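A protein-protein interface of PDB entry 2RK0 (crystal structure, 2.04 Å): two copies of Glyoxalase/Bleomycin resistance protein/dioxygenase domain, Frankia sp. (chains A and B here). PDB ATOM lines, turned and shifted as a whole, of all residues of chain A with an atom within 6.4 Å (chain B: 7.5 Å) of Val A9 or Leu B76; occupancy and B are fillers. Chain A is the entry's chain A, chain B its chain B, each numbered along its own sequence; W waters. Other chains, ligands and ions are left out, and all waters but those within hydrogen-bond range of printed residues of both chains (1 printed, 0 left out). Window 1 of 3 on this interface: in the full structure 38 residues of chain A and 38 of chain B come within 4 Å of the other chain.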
ATOM      1  N   VAL A   6     -16.674 -31.534 -19.314  1.00  0.00           N
ATOM      2  CA  VAL A   6     -16.932 -30.246 -19.937  1.00  0.00           C
ATOM      3  C   VAL A   6     -18.412 -30.037 -20.228  1.00  0.00           C
ATOM      4  O   VAL A   6     -19.034 -30.833 -20.924  1.00  0.00           O
ATOM      5  CB  VAL A   6     -16.148 -30.090 -21.272  1.00  0.00           C
ATOM      6  CG1 VAL A   6     -16.461 -28.743 -21.910  1.00  0.00           C
ATOM      7  CG2 VAL A   6     -14.649 -30.216 -21.022  1.00  0.00           C
ATOM      8  N   SER A   7     -18.976 -28.964 -19.687  1.00  0.00           N
ATOM      9  CA  SER A   7     -20.377 -28.642 -19.924  1.00  0.00           C
ATOM     10  C   SER A   7     -20.467 -28.051 -21.334  1.00  0.00           C
ATOM     11  O   SER A   7     -21.360 -28.380 -22.120  1.00  0.00           O
ATOM     12  CB  SER A   7     -20.856 -27.626 -18.891  1.00  0.00           C
ATOM     13  OG  SER A   7     -22.217 -27.316 -19.104  1.00  0.00           O
ATOM     14  N   HIS A   8     -19.527 -27.168 -21.643  1.00  0.00           N
ATOM     15  CA  HIS A   8     -19.462 -26.557 -22.960  1.00  0.00           C
ATOM     16  C   HIS A   8     -18.248 -25.663 -23.102  1.00  0.00           C
ATOM     17  O   HIS A   8     -17.643 -25.235 -22.119  1.00  0.00           O
ATOM     18  CB  HIS A   8     -20.725 -25.749 -23.266  1.00  0.00           C
ATOM     19  CG  HIS A   8     -20.904 -24.542 -22.404  1.00  0.00           C
ATOM     20  ND1 HIS A   8     -21.703 -24.541 -21.279  1.00  0.00           N
ATOM     21  CD2 HIS A   8     -20.411 -23.284 -22.517  1.00  0.00           C
ATOM     22  CE1 HIS A   8     -21.697 -23.336 -20.738  1.00  0.00           C
ATOM     23  NE2 HIS A   8     -20.921 -22.555 -21.472  1.00  0.00           N
ATOM     24  N   VAL A   9     -17.887 -25.391 -24.344  1.00  0.00           N
ATOM     25  CA  VAL A   9     -16.745 -24.538 -24.610  1.00  0.00           C
ATOM     26  C   VAL A   9     -17.233 -23.324 -25.364  1.00  0.00           C
ATOM     27  O   VAL A   9     -17.911 -23.445 -26.380  1.00  0.00           O
ATOM     28  CB  VAL A   9     -15.694 -25.251 -25.469  1.00  0.00           C
ATOM     29  CG1 VAL A   9     -14.498 -24.325 -25.688  1.00  0.00           C
ATOM     30  CG2 VAL A   9     -15.261 -26.542 -24.793  1.00  0.00           C
ATOM     31  N   SER A  10     -16.902 -22.148 -24.857  1.00  0.00           N
ATOM     32  CA  SER A  10     -17.307 -20.933 -25.531  1.00  0.00           C
ATOM     33  C   SER A  10     -16.067 -20.342 -26.192  1.00  0.00           C
ATOM     34  O   SER A  10     -15.075 -20.056 -25.521  1.00  0.00           O
ATOM     35  CB  SER A  10     -17.909 -19.953 -24.525  1.00  0.00           C
ATOM     36  OG  SER A  10     -18.440 -18.833 -25.202  1.00  0.00           O
ATOM     37  N   LEU A  11     -16.127 -20.181 -27.510  1.00  0.00           N
ATOM     38  CA  LEU A  11     -15.017 -19.643 -28.284  1.00  0.00           C
ATOM     39  C   LEU A  11     -15.293 -18.230 -28.769  1.00  0.00           C
ATOM     40  O   LEU A  11     -16.415 -17.900 -29.151  1.00  0.00           O
ATOM     41  CB  LEU A  11     -14.743 -20.524 -29.507  1.00  0.00           C
ATOM     42  CG  LEU A  11     -14.442 -22.005 -29.261  1.00  0.00           C
ATOM     43  CD1 LEU A  11     -14.141 -22.674 -30.595  1.00  0.00           C
ATOM     44  CD2 LEU A  11     -13.252 -22.157 -28.308  1.00  0.00           C
ATOM     45  N   LEU A  51     -20.953 -32.735 -27.408  1.00  0.00           N
ATOM     46  CA  LEU A  51     -20.245 -31.541 -26.937  1.00  0.00           C
ATOM     47  C   LEU A  51     -20.875 -30.235 -27.391  1.00  0.00           C
ATOM     48  O   LEU A  51     -21.110 -30.021 -28.582  1.00  0.00           O
ATOM     49  CB  LEU A  51     -18.777 -31.554 -27.379  1.00  0.00           C
ATOM     50  CG  LEU A  51     -17.995 -30.303 -26.948  1.00  0.00           C
ATOM     51  CD1 LEU A  51     -17.995 -30.174 -25.432  1.00  0.00           C
ATOM     52  CD2 LEU A  51     -16.576 -30.377 -27.471  1.00  0.00           C
ATOM     53  N   SER A  52     -21.150 -29.363 -26.426  1.00  0.00           N
ATOM     54  CA  SER A  52     -21.735 -28.061 -26.711  1.00  0.00           C
ATOM     55  C   SER A  52     -20.639 -27.040 -26.957  1.00  0.00           C
ATOM     56  O   SER A  52     -19.696 -26.926 -26.175  1.00  0.00           O
ATOM     57  CB  SER A  52     -22.602 -27.569 -25.544  1.00  0.00           C
ATOM     58  OG  SER A  52     -23.947 -27.992 -25.666  1.00  0.00           O
ATOM     59  N   ILE A  53     -20.772 -26.301 -28.049  1.00  0.00           N
ATOM     60  CA  ILE A  53     -19.817 -25.262 -28.383  1.00  0.00           C
ATOM     61  C   ILE A  53     -20.567 -23.975 -28.669  1.00  0.00           C
ATOM     62  O   ILE A  53     -21.465 -23.933 -29.518  1.00  0.00           O
ATOM     63  CB  ILE A  53     -18.976 -25.614 -29.622  1.00  0.00           C
ATOM     64  CG1 ILE A  53     -18.082 -26.809 -29.315  1.00  0.00           C
ATOM     65  CG2 ILE A  53     -18.121 -24.412 -30.028  1.00  0.00           C
ATOM     66  CD1 ILE A  53     -17.224 -27.221 -30.466  1.00  0.00           C
ATOM     67  N   VAL A  54     -20.199 -22.925 -27.948  1.00  0.00           N
ATOM     68  CA  VAL A  54     -20.829 -21.633 -28.137  1.00  0.00           C
ATOM     69  C   VAL A  54     -19.830 -20.732 -28.851  1.00  0.00           C
ATOM     70  O   VAL A  54     -18.684 -20.609 -28.424  1.00  0.00           O
ATOM     71  CB  VAL A  54     -21.217 -20.986 -26.788  1.00  0.00           C
ATOM     72  CG1 VAL A  54     -21.960 -19.679 -27.039  1.00  0.00           C
ATOM     73  CG2 VAL A  54     -22.084 -21.957 -25.967  1.00  0.00           C
ATOM     74  N   LEU A  55     -20.265 -20.139 -29.959  1.00  0.00           N
ATOM     75  CA  LEU A  55     -19.427 -19.228 -30.734  1.00  0.00           C
ATOM     76  C   LEU A  55     -19.829 -17.834 -30.280  1.00  0.00           C
ATOM     77  O   LEU A  55     -21.016 -17.521 -30.191  1.00  0.00           O
ATOM     78  CB  LEU A  55     -19.687 -19.411 -32.232  1.00  0.00           C
ATOM     79  CG  LEU A  55     -19.475 -20.848 -32.730  1.00  0.00           C
ATOM     80  CD1 LEU A  55     -19.761 -20.962 -34.222  1.00  0.00           C
ATOM     81  CD2 LEU A  55     -18.049 -21.266 -32.443  1.00  0.00           C
ATOM     82  N   LEU A  73      -6.777 -20.402 -24.384  1.00  0.00           N
ATOM     83  CA  LEU A  73      -6.679 -21.682 -25.083  1.00  0.00           C
ATOM     84  C   LEU A  73      -5.371 -21.883 -25.862  1.00  0.00           C
ATOM     85  O   LEU A  73      -4.964 -21.018 -26.633  1.00  0.00           O
ATOM     86  CB  LEU A  73      -7.855 -21.831 -26.058  1.00  0.00           C
ATOM     87  CG  LEU A  73      -7.962 -23.154 -26.830  1.00  0.00           C
ATOM     88  CD1 LEU A  73      -8.252 -24.301 -25.874  1.00  0.00           C
ATOM     89  CD2 LEU A  73      -9.073 -23.058 -27.868  1.00  0.00           C
ATOM     90  N   LEU A  76      -7.641 -27.166 -28.579  1.00  0.00           N
ATOM     91  CA  LEU A  76      -8.740 -28.031 -28.152  1.00  0.00           C
ATOM     92  C   LEU A  76      -8.718 -29.340 -28.951  1.00  0.00           C
ATOM     93  O   LEU A  76      -8.773 -29.325 -30.175  1.00  0.00           O
ATOM     94  CB  LEU A  76     -10.072 -27.313 -28.367  1.00  0.00           C
ATOM     95  CG  LEU A  76     -11.355 -28.055 -27.990  1.00  0.00           C
ATOM     96  CD1 LEU A  76     -11.310 -28.486 -26.524  1.00  0.00           C
ATOM     97  CD2 LEU A  76     -12.540 -27.141 -28.246  1.00  0.00           C
ATOM     98  N   VAL B   6     -14.539 -34.450 -25.867  1.00  0.00           N
ATOM     99  CA  VAL B   6     -13.244 -33.810 -25.662  1.00  0.00           C
ATOM    100  C   VAL B   6     -12.165 -34.776 -25.183  1.00  0.00           C
ATOM    101  O   VAL B   6     -12.310 -35.413 -24.143  1.00  0.00           O
ATOM    102  CB  VAL B   6     -13.352 -32.666 -24.634  1.00  0.00           C
ATOM    103  CG1 VAL B   6     -11.973 -32.083 -24.354  1.00  0.00           C
ATOM    104  CG2 VAL B   6     -14.299 -31.595 -25.151  1.00  0.00           C
ATOM    105  N   VAL B   9      -8.138 -30.565 -23.130  1.00  0.00           N
ATOM    106  CA  VAL B   9      -8.087 -29.136 -23.368  1.00  0.00           C
ATOM    107  C   VAL B   9      -6.703 -28.686 -22.933  1.00  0.00           C
ATOM    108  O   VAL B   9      -6.232 -29.056 -21.857  1.00  0.00           O
ATOM    109  CB  VAL B   9      -9.140 -28.378 -22.521  1.00  0.00           C
ATOM    110  CG1 VAL B   9      -9.041 -26.874 -22.785  1.00  0.00           C
ATOM    111  CG2 VAL B   9     -10.535 -28.890 -22.850  1.00  0.00           C
ATOM    112  N   SER B  10      -6.042 -27.899 -23.771  1.00  0.00           N
ATOM    113  CA  SER B  10      -4.718 -27.400 -23.428  1.00  0.00           C
ATOM    114  C   SER B  10      -4.860 -25.902 -23.185  1.00  0.00           C
ATOM    115  O   SER B  10      -5.319 -25.171 -24.060  1.00  0.00           O
ATOM    116  CB  SER B  10      -3.734 -27.671 -24.568  1.00  0.00           C
ATOM    117  OG  SER B  10      -2.407 -27.389 -24.172  1.00  0.00           O
ATOM    118  N   LEU B  11      -4.477 -25.462 -21.988  1.00  0.00           N
ATOM    119  CA  LEU B  11      -4.564 -24.053 -21.604  1.00  0.00           C
ATOM    120  C   LEU B  11      -3.183 -23.426 -21.439  1.00  0.00           C
ATOM    121  O   LEU B  11      -2.292 -24.017 -20.831  1.00  0.00           O
ATOM    122  CB  LEU B  11      -5.321 -23.908 -20.280  1.00  0.00           C
ATOM    123  CG  LEU B  11      -6.766 -24.420 -20.189  1.00  0.00           C
ATOM    124  CD1 LEU B  11      -7.266 -24.274 -18.754  1.00  0.00           C
ATOM    125  CD2 LEU B  11      -7.652 -23.631 -21.135  1.00  0.00           C
ATOM    126  N   TYR B  23      -4.712 -25.080  -9.996  1.00  0.00           N
ATOM    127  CA  TYR B  23      -5.639 -26.084 -10.508  1.00  0.00           C
ATOM    128  C   TYR B  23      -5.757 -27.271  -9.563  1.00  0.00           C
ATOM    129  O   TYR B  23      -6.836 -27.834  -9.399  1.00  0.00           O
ATOM    130  CB  TYR B  23      -5.228 -26.531 -11.922  1.00  0.00           C
ATOM    131  CG  TYR B  23      -5.704 -25.573 -12.993  1.00  0.00           C
ATOM    132  CD1 TYR B  23      -5.030 -24.383 -13.255  1.00  0.00           C
ATOM    133  CD2 TYR B  23      -6.913 -25.796 -13.647  1.00  0.00           C
ATOM    134  CE1 TYR B  23      -5.561 -23.420 -14.141  1.00  0.00           C
ATOM    135  CE2 TYR B  23      -7.450 -24.859 -14.522  1.00  0.00           C
ATOM    136  CZ  TYR B  23      -6.781 -23.674 -14.763  1.00  0.00           C
ATOM    137  OH  TYR B  23      -7.381 -22.741 -15.579  1.00  0.00           O
ATOM    138  N   LEU B  27      -9.550 -27.264  -8.278  1.00  0.00           N
ATOM    139  CA  LEU B  27     -10.318 -28.291  -8.979  1.00  0.00           C
ATOM    140  C   LEU B  27      -9.882 -29.728  -8.761  1.00  0.00           C
ATOM    141  O   LEU B  27     -10.409 -30.626  -9.412  1.00  0.00           O
ATOM    142  CB  LEU B  27     -10.292 -28.003 -10.482  1.00  0.00           C
ATOM    143  CG  LEU B  27     -10.733 -26.593 -10.897  1.00  0.00           C
ATOM    144  CD1 LEU B  27     -10.517 -26.386 -12.390  1.00  0.00           C
ATOM    145  CD2 LEU B  27     -12.198 -26.399 -10.540  1.00  0.00           C
ATOM    146  N   LEU B  47      -8.709 -34.163 -14.164  1.00  0.00           N
ATOM    147  CA  LEU B  47      -9.646 -33.745 -13.129  1.00  0.00           C
ATOM    148  C   LEU B  47     -10.476 -34.922 -12.658  1.00  0.00           C
ATOM    149  O   LEU B  47     -10.489 -35.984 -13.292  1.00  0.00           O
ATOM    150  CB  LEU B  47     -10.615 -32.699 -13.671  1.00  0.00           C
ATOM    151  CG  LEU B  47     -10.063 -31.375 -14.187  1.00  0.00           C
ATOM    152  CD1 LEU B  47     -11.215 -30.556 -14.745  1.00  0.00           C
ATOM    153  CD2 LEU B  47      -9.354 -30.636 -13.066  1.00  0.00           C
ATOM    154  N   LEU B  51     -11.499 -35.857 -16.968  1.00  0.00           N
ATOM    155  CA  LEU B  51     -11.132 -34.891 -18.008  1.00  0.00           C
ATOM    156  C   LEU B  51      -9.652 -34.511 -17.974  1.00  0.00           C
ATOM    157  O   LEU B  51      -9.117 -34.171 -16.922  1.00  0.00           O
ATOM    158  CB  LEU B  51     -11.967 -33.618 -17.887  1.00  0.00           C
ATOM    159  CG  LEU B  51     -11.610 -32.498 -18.870  1.00  0.00           C
ATOM    160  CD1 LEU B  51     -11.896 -32.951 -20.302  1.00  0.00           C
ATOM    161  CD2 LEU B  51     -12.416 -31.253 -18.539  1.00  0.00           C
ATOM    162  N   ILE B  53      -6.558 -32.088 -18.692  1.00  0.00           N
ATOM    163  CA  ILE B  53      -6.237 -30.669 -18.837  1.00  0.00           C
ATOM    164  C   ILE B  53      -4.721 -30.499 -18.851  1.00  0.00           C
ATOM    165  O   ILE B  53      -4.023 -30.881 -17.904  1.00  0.00           O
ATOM    166  CB  ILE B  53      -6.782 -29.812 -17.660  1.00  0.00           C
ATOM    167  CG1 ILE B  53      -8.307 -29.921 -17.562  1.00  0.00           C
ATOM    168  CG2 ILE B  53      -6.361 -28.358 -17.854  1.00  0.00           C
ATOM    169  CD1 ILE B  53      -9.045 -29.482 -18.805  1.00  0.00           C
ATOM    170  N   PHE B  66      -5.288 -13.205 -19.565  1.00  0.00           N
ATOM    171  CA  PHE B  66      -6.310 -13.705 -20.472  1.00  0.00           C
ATOM    172  C   PHE B  66      -7.194 -12.523 -20.895  1.00  0.00           C
ATOM    173  O   PHE B  66      -7.432 -11.615 -20.103  1.00  0.00           O
ATOM    174  CB  PHE B  66      -7.152 -14.742 -19.729  1.00  0.00           C
ATOM    175  CG  PHE B  66      -8.422 -15.126 -20.433  1.00  0.00           C
ATOM    176  CD1 PHE B  66      -8.412 -16.071 -21.453  1.00  0.00           C
ATOM    177  CD2 PHE B  66      -9.636 -14.576 -20.040  1.00  0.00           C
ATOM    178  CE1 PHE B  66      -9.602 -16.467 -22.069  1.00  0.00           C
ATOM    179  CE2 PHE B  66     -10.827 -14.960 -20.646  1.00  0.00           C
ATOM    180  CZ  PHE B  66     -10.811 -15.911 -21.662  1.00  0.00           C
ATOM    181  N   GLY B  72     -10.109 -17.216 -29.609  1.00  0.00           N
ATOM    182  CA  GLY B  72      -9.661 -18.368 -28.851  1.00  0.00           C
ATOM    183  C   GLY B  72     -10.721 -18.685 -27.818  1.00  0.00           C
ATOM    184  O   GLY B  72     -11.903 -18.786 -28.148  1.00  0.00           O
ATOM    185  N   LEU B  73     -10.308 -18.826 -26.565  1.00  0.00           N
ATOM    186  CA  LEU B  73     -11.251 -19.127 -25.505  1.00  0.00           C
ATOM    187  C   LEU B  73     -11.999 -17.895 -25.014  1.00  0.00           C
ATOM    188  O   LEU B  73     -11.398 -16.847 -24.763  1.00  0.00           O
ATOM    189  CB  LEU B  73     -10.532 -19.762 -24.308  1.00  0.00           C
ATOM    190  CG  LEU B  73     -11.449 -20.233 -23.172  1.00  0.00           C
ATOM    191  CD1 LEU B  73     -12.257 -21.447 -23.634  1.00  0.00           C
ATOM    192  CD2 LEU B  73     -10.611 -20.613 -21.951  1.00  0.00           C
ATOM    193  N   ASP B  74     -13.317 -18.035 -24.894  1.00  0.00           N
ATOM    194  CA  ASP B  74     -14.173 -16.985 -24.364  1.00  0.00           C
ATOM    195  C   ASP B  74     -14.265 -17.389 -22.888  1.00  0.00           C
ATOM    196  O   ASP B  74     -14.044 -16.583 -21.989  1.00  0.00           O
ATOM    197  CB  ASP B  74     -15.544 -17.027 -25.029  1.00  0.00           C
ATOM    198  CG  ASP B  74     -16.521 -16.019 -24.424  1.00  0.00           C
ATOM    199  OD1 ASP B  74     -16.261 -14.802 -24.494  1.00  0.00           O
ATOM    200  OD2 ASP B  74     -17.550 -16.456 -23.881  1.00  0.00           O
ATOM    201  N   HIS B  75     -14.595 -18.657 -22.658  1.00  0.00           N
ATOM    202  CA  HIS B  75     -14.643 -19.230 -21.315  1.00  0.00           C
ATOM    203  C   HIS B  75     -14.879 -20.732 -21.388  1.00  0.00           C
ATOM    204  O   HIS B  75     -15.475 -21.227 -22.348  1.00  0.00           O
ATOM    205  CB  HIS B  75     -15.678 -18.521 -20.418  1.00  0.00           C
ATOM    206  CG  HIS B  75     -17.108 -18.767 -20.791  1.00  0.00           C
ATOM    207  ND1 HIS B  75     -17.746 -19.961 -20.547  1.00  0.00           N
ATOM    208  CD2 HIS B  75     -18.039 -17.940 -21.326  1.00  0.00           C
ATOM    209  CE1 HIS B  75     -19.017 -19.861 -20.911  1.00  0.00           C
ATOM    210  NE2 HIS B  75     -19.217 -18.647 -21.384  1.00  0.00           N
ATOM    211  N   LEU B  76     -14.354 -21.453 -20.398  1.00  0.00           N
ATOM    212  CA  LEU B  76     -14.495 -22.903 -20.336  1.00  0.00           C
ATOM    213  C   LEU B  76     -15.474 -23.295 -19.231  1.00  0.00           C
ATOM    214  O   LEU B  76     -15.322 -22.884 -18.083  1.00  0.00           O
ATOM    215  CB  LEU B  76     -13.134 -23.554 -20.078  1.00  0.00           C
ATOM    216  CG  LEU B  76     -13.161 -25.075 -19.970  1.00  0.00           C
ATOM    217  CD1 LEU B  76     -13.716 -25.677 -21.254  1.00  0.00           C
ATOM    218  CD2 LEU B  76     -11.757 -25.585 -19.697  1.00  0.00           C
ATOM    219  N   SER B  77     -16.473 -24.101 -19.572  1.00  0.00           N
ATOM    220  CA  SER B  77     -17.468 -24.483 -18.587  1.00  0.00           C
ATOM    221  C   SER B  77     -17.441 -25.954 -18.188  1.00  0.00           C
ATOM    222  O   SER B  77     -17.622 -26.836 -19.023  1.00  0.00           O
ATOM    223  CB  SER B  77     -18.857 -24.107 -19.104  1.00  0.00           C
ATOM    224  OG  SER B  77     -19.828 -24.265 -18.085  1.00  0.00           O
ATOM    225  N   PHE B  78     -17.207 -26.201 -16.901  1.00  0.00           N
ATOM    226  CA  PHE B  78     -17.165 -27.558 -16.362  1.00  0.00           C
ATOM    227  C   PHE B  78     -18.536 -27.939 -15.806  1.00  0.00           C
ATOM    228  O   PHE B  78     -19.240 -27.111 -15.223  1.00  0.00           O
ATOM    229  CB  PHE B  78     -16.140 -27.654 -15.231  1.00  0.00           C
ATOM    230  CG  PHE B  78     -14.740 -27.311 -15.643  1.00  0.00           C
ATOM    231  CD1 PHE B  78     -14.031 -28.141 -16.503  1.00  0.00           C
ATOM    232  CD2 PHE B  78     -14.123 -26.157 -15.158  1.00  0.00           C
ATOM    233  CE1 PHE B  78     -12.728 -27.832 -16.875  1.00  0.00           C
ATOM    234  CE2 PHE B  78     -12.820 -25.831 -15.520  1.00  0.00           C
ATOM    235  CZ  PHE B  78     -12.117 -26.669 -16.381  1.00  0.00           C
ATOM    236  N   LEU B 112     -21.521 -21.044 -11.586  1.00  0.00           N
ATOM    237  CA  LEU B 112     -20.541 -20.414 -10.724  1.00  0.00           C
ATOM    238  C   LEU B 112     -19.424 -19.963 -11.665  1.00  0.00           C
ATOM    239  O   LEU B 112     -18.745 -20.793 -12.261  1.00  0.00           O
ATOM    240  CB  LEU B 112     -20.004 -21.424  -9.700  1.00  0.00           C
ATOM    241  CG  LEU B 112     -18.778 -20.992  -8.884  1.00  0.00           C
ATOM    242  CD1 LEU B 112     -19.088 -19.712  -8.119  1.00  0.00           C
ATOM    243  CD2 LEU B 112     -18.368 -22.118  -7.927  1.00  0.00           C
ATOM    244  N   PHE B 114     -15.837 -18.090 -12.287  1.00  0.00           N
ATOM    245  CA  PHE B 114     -14.615 -17.721 -11.588  1.00  0.00           C
ATOM    246  C   PHE B 114     -13.419 -17.515 -12.525  1.00  0.00           C
ATOM    247  O   PHE B 114     -13.496 -17.803 -13.719  1.00  0.00           O
ATOM    248  CB  PHE B 114     -14.297 -18.772 -10.520  1.00  0.00           C
ATOM    249  CG  PHE B 114     -14.225 -20.180 -11.045  1.00  0.00           C
ATOM    250  CD1 PHE B 114     -12.991 -20.813 -11.203  1.00  0.00           C
ATOM    251  CD2 PHE B 114     -15.390 -20.892 -11.347  1.00  0.00           C
ATOM    252  CE1 PHE B 114     -12.911 -22.133 -11.647  1.00  0.00           C
ATOM    253  CE2 PHE B 114     -15.324 -22.215 -11.793  1.00  0.00           C
ATOM    254  CZ  PHE B 114     -14.081 -22.839 -11.943  1.00  0.00           C
ATOM    255  N   ILE B 120      -8.105 -16.418 -16.543  1.00  0.00           N
ATOM    256  CA  ILE B 120      -8.850 -17.192 -17.530  1.00  0.00           C
ATOM    257  C   ILE B 120     -10.270 -17.406 -17.009  1.00  0.00           C
ATOM    258  O   ILE B 120     -10.463 -17.821 -15.867  1.00  0.00           O
ATOM    259  CB  ILE B 120      -8.194 -18.557 -17.803  1.00  0.00           C
ATOM    260  CG1 ILE B 120      -6.817 -18.350 -18.450  1.00  0.00           C
ATOM    261  CG2 ILE B 120      -9.094 -19.386 -18.709  1.00  0.00           C
ATOM    262  CD1 ILE B 120      -6.060 -19.640 -18.734  1.00  0.00           C
ATOM    263  N   ALA B 121     -11.260 -17.103 -17.845  1.00  0.00           N
ATOM    264  CA  ALA B 121     -12.661 -17.241 -17.464  1.00  0.00           C
ATOM    265  C   ALA B 121     -13.108 -18.702 -17.424  1.00  0.00           C
ATOM    266  O   ALA B 121     -13.072 -19.405 -18.428  1.00  0.00           O
ATOM    267  CB  ALA B 121     -13.549 -16.444 -18.426  1.00  0.00           C
ATOM    268  N   LEU B 122     -13.538 -19.144 -16.249  1.00  0.00           N
ATOM    269  CA  LEU B 122     -13.992 -20.514 -16.068  1.00  0.00           C
ATOM    270  C   LEU B 122     -15.366 -20.511 -15.416  1.00  0.00           C
ATOM    271  O   LEU B 122     -15.753 -19.533 -14.778  1.00  0.00           O
ATOM    272  CB  LEU B 122     -13.018 -21.280 -15.176  1.00  0.00           C
ATOM    273  CG  LEU B 122     -11.545 -21.350 -15.591  1.00  0.00           C
ATOM    274  CD1 LEU B 122     -10.736 -22.042 -14.497  1.00  0.00           C
ATOM    275  CD2 LEU B 122     -11.419 -22.091 -16.905  1.00  0.00           C
ATOM    276  N   GLU B 123     -16.092 -21.608 -15.581  1.00  0.00           N
ATOM    277  CA  GLU B 123     -17.414 -21.753 -14.989  1.00  0.00           C
ATOM    278  C   GLU B 123     -17.646 -23.208 -14.599  1.00  0.00           C
ATOM    279  O   GLU B 123     -17.058 -24.128 -15.173  1.00  0.00           O
ATOM    280  CB  GLU B 123     -18.525 -21.338 -15.962  1.00  0.00           C
ATOM    281  CG  GLU B 123     -18.514 -19.886 -16.404  1.00  0.00           C
ATOM    282  CD  GLU B 123     -19.714 -19.545 -17.282  1.00  0.00           C
ATOM    283  OE1 GLU B 123     -20.304 -20.471 -17.879  1.00  0.00           O
ATOM    284  OE2 GLU B 123     -20.059 -18.352 -17.389  1.00  0.00           O
ATOM    285  N   ALA B 124     -18.504 -23.388 -13.606  1.00  0.00           N
ATOM    286  CA  ALA B 124     -18.894 -24.699 -13.120  1.00  0.00           C
ATOM    287  C   ALA B 124     -20.405 -24.611 -13.164  1.00  0.00           C
ATOM    288  O   ALA B 124     -21.000 -23.701 -12.580  1.00  0.00           O
ATOM    289  CB  ALA B 124     -18.427 -24.902 -11.696  1.00  0.00           C
HETATM  290  O   HOH W   1      -7.590 -17.934 -25.886  1.00  0.00           O
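The backbone carbonyl oxygen (O) of Ser B77 sits at hydrogen-bond distance from the backbone NH (N) of Ser A7 (2.6 Å).
The backbone NH (N) of Ser B77 sits at hydrogen-bond distance from the backbone carbonyl oxygen (O) of His A8, at 3.0 Å.
The backbone carbonyl oxygen (O) of Ser A10 lies within hydrogen-bond range of the backbone NH (N) of Asp B74 (2.8 Å).
The backbone NH (N) of Ser A10 sits at hydrogen-bond distance from the backbone carbonyl oxygen (O) of His B75 (3.0 Å).
N of Val A9 lies within hydrogen-bond range of O of Ser A52, at 3.0 Å.
The backbone carbonyl oxygen (O) of Val A9 is in hydrogen-bond range of the backbone NH (N) of Val A54 (2.8 Å).
The backbone carbonyl oxygen of Val A54 sits at hydrogen-bond distance from the backbone NH of Leu A11 (2.7 Å).
The backbone carbonyl oxygen (O) of Ala B121 sits at hydrogen-bond distance from the backbone NH (N) of Leu B76 (3.1 Å).
The backbone NH (N) of Glu B123 lies within hydrogen-bond range of the backbone carbonyl oxygen (O) of Leu B76 (2.9 Å).
N of Phe B78 lies within hydrogen-bond range of O of Glu B123, at 2.7 Å.
Among the printed residues, merely in contact across the chains: Val A6 with Leu B51, Val A6 with Ser B77, Ser A7 with Phe B78, His A8 with His B75, Val A9 with Leu B76, Ser A10 with Leu B73, Leu A11 with Gly B72, Leu A11 with Asp B74, Leu A51 with Val B6, Leu A73 with Ser B10, Leu A73 with Leu B73 and Leu A76 with Val B9.
Val A9 touches just one residue of chain B: Leu B76 (3.96 Å).
Of the printed residues of chain B, Ser A10 touches Leu B73 (3.7 Å), Asp B74 (2.8 Å) and His B75 (3.0 Å).
Printed residues of chain A within 4 Å of Leu B51: Val A6 (3.5 Å).
Phe B66 touches none of the printed residues of chain A.
Printed residues of chain A within 4 Å of Gly B72: Leu A11.
Of the printed residues of chain A, Leu B73 touches Ser A10 and Leu A73.
Leu B76 touches just one residue of chain A: Val A9 (3.96 Å).
Ala B121 touches none of the printed residues of chain A.
The nearest residue of chain A that does not touch Leu B76 is His A8 (4.05 Å).
The nearest printed residue of chain A that does not touch Asp B74 is Val A54 (5.8 Å).
Of the 13 printed residues of chain A, 9 touch a printed residue of chain B.
Printed residues of chain B that touch a printed residue of chain A: Val B6, Val B9, Ser B10, Leu B51, Gly B72, Leu B73, Asp B74, His B75, Leu B76, Ser B77 and Phe B78.
Hydrophobic or aromatic side chains of chain B that line the printed part of chain A: Val B6, Val B9, Leu B51, Leu B73, His B75 and Leu B76.
Val A6 touches Leu B51, and with the chains exchanged Leu A51 touches Val B6.
Val A9 touches Leu B76, and with the chains exchanged Leu A76 touches Val B9.
Ser A10 touches Leu B73, and with the chains exchanged Leu A73 touches Ser B10.
Leu B73 touches its own counterpart, Leu A73.
Positions printed for both chains: 6, 9, 10, 11, 51, 53, 73 and 76.
Of the 16 pairs that touch across the chains among the printed residues, 7 have their exchanged pair printed and touching as well.
Water W1 lies within hydrogen-bond range of N of Leu B73 and N of Leu A73.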
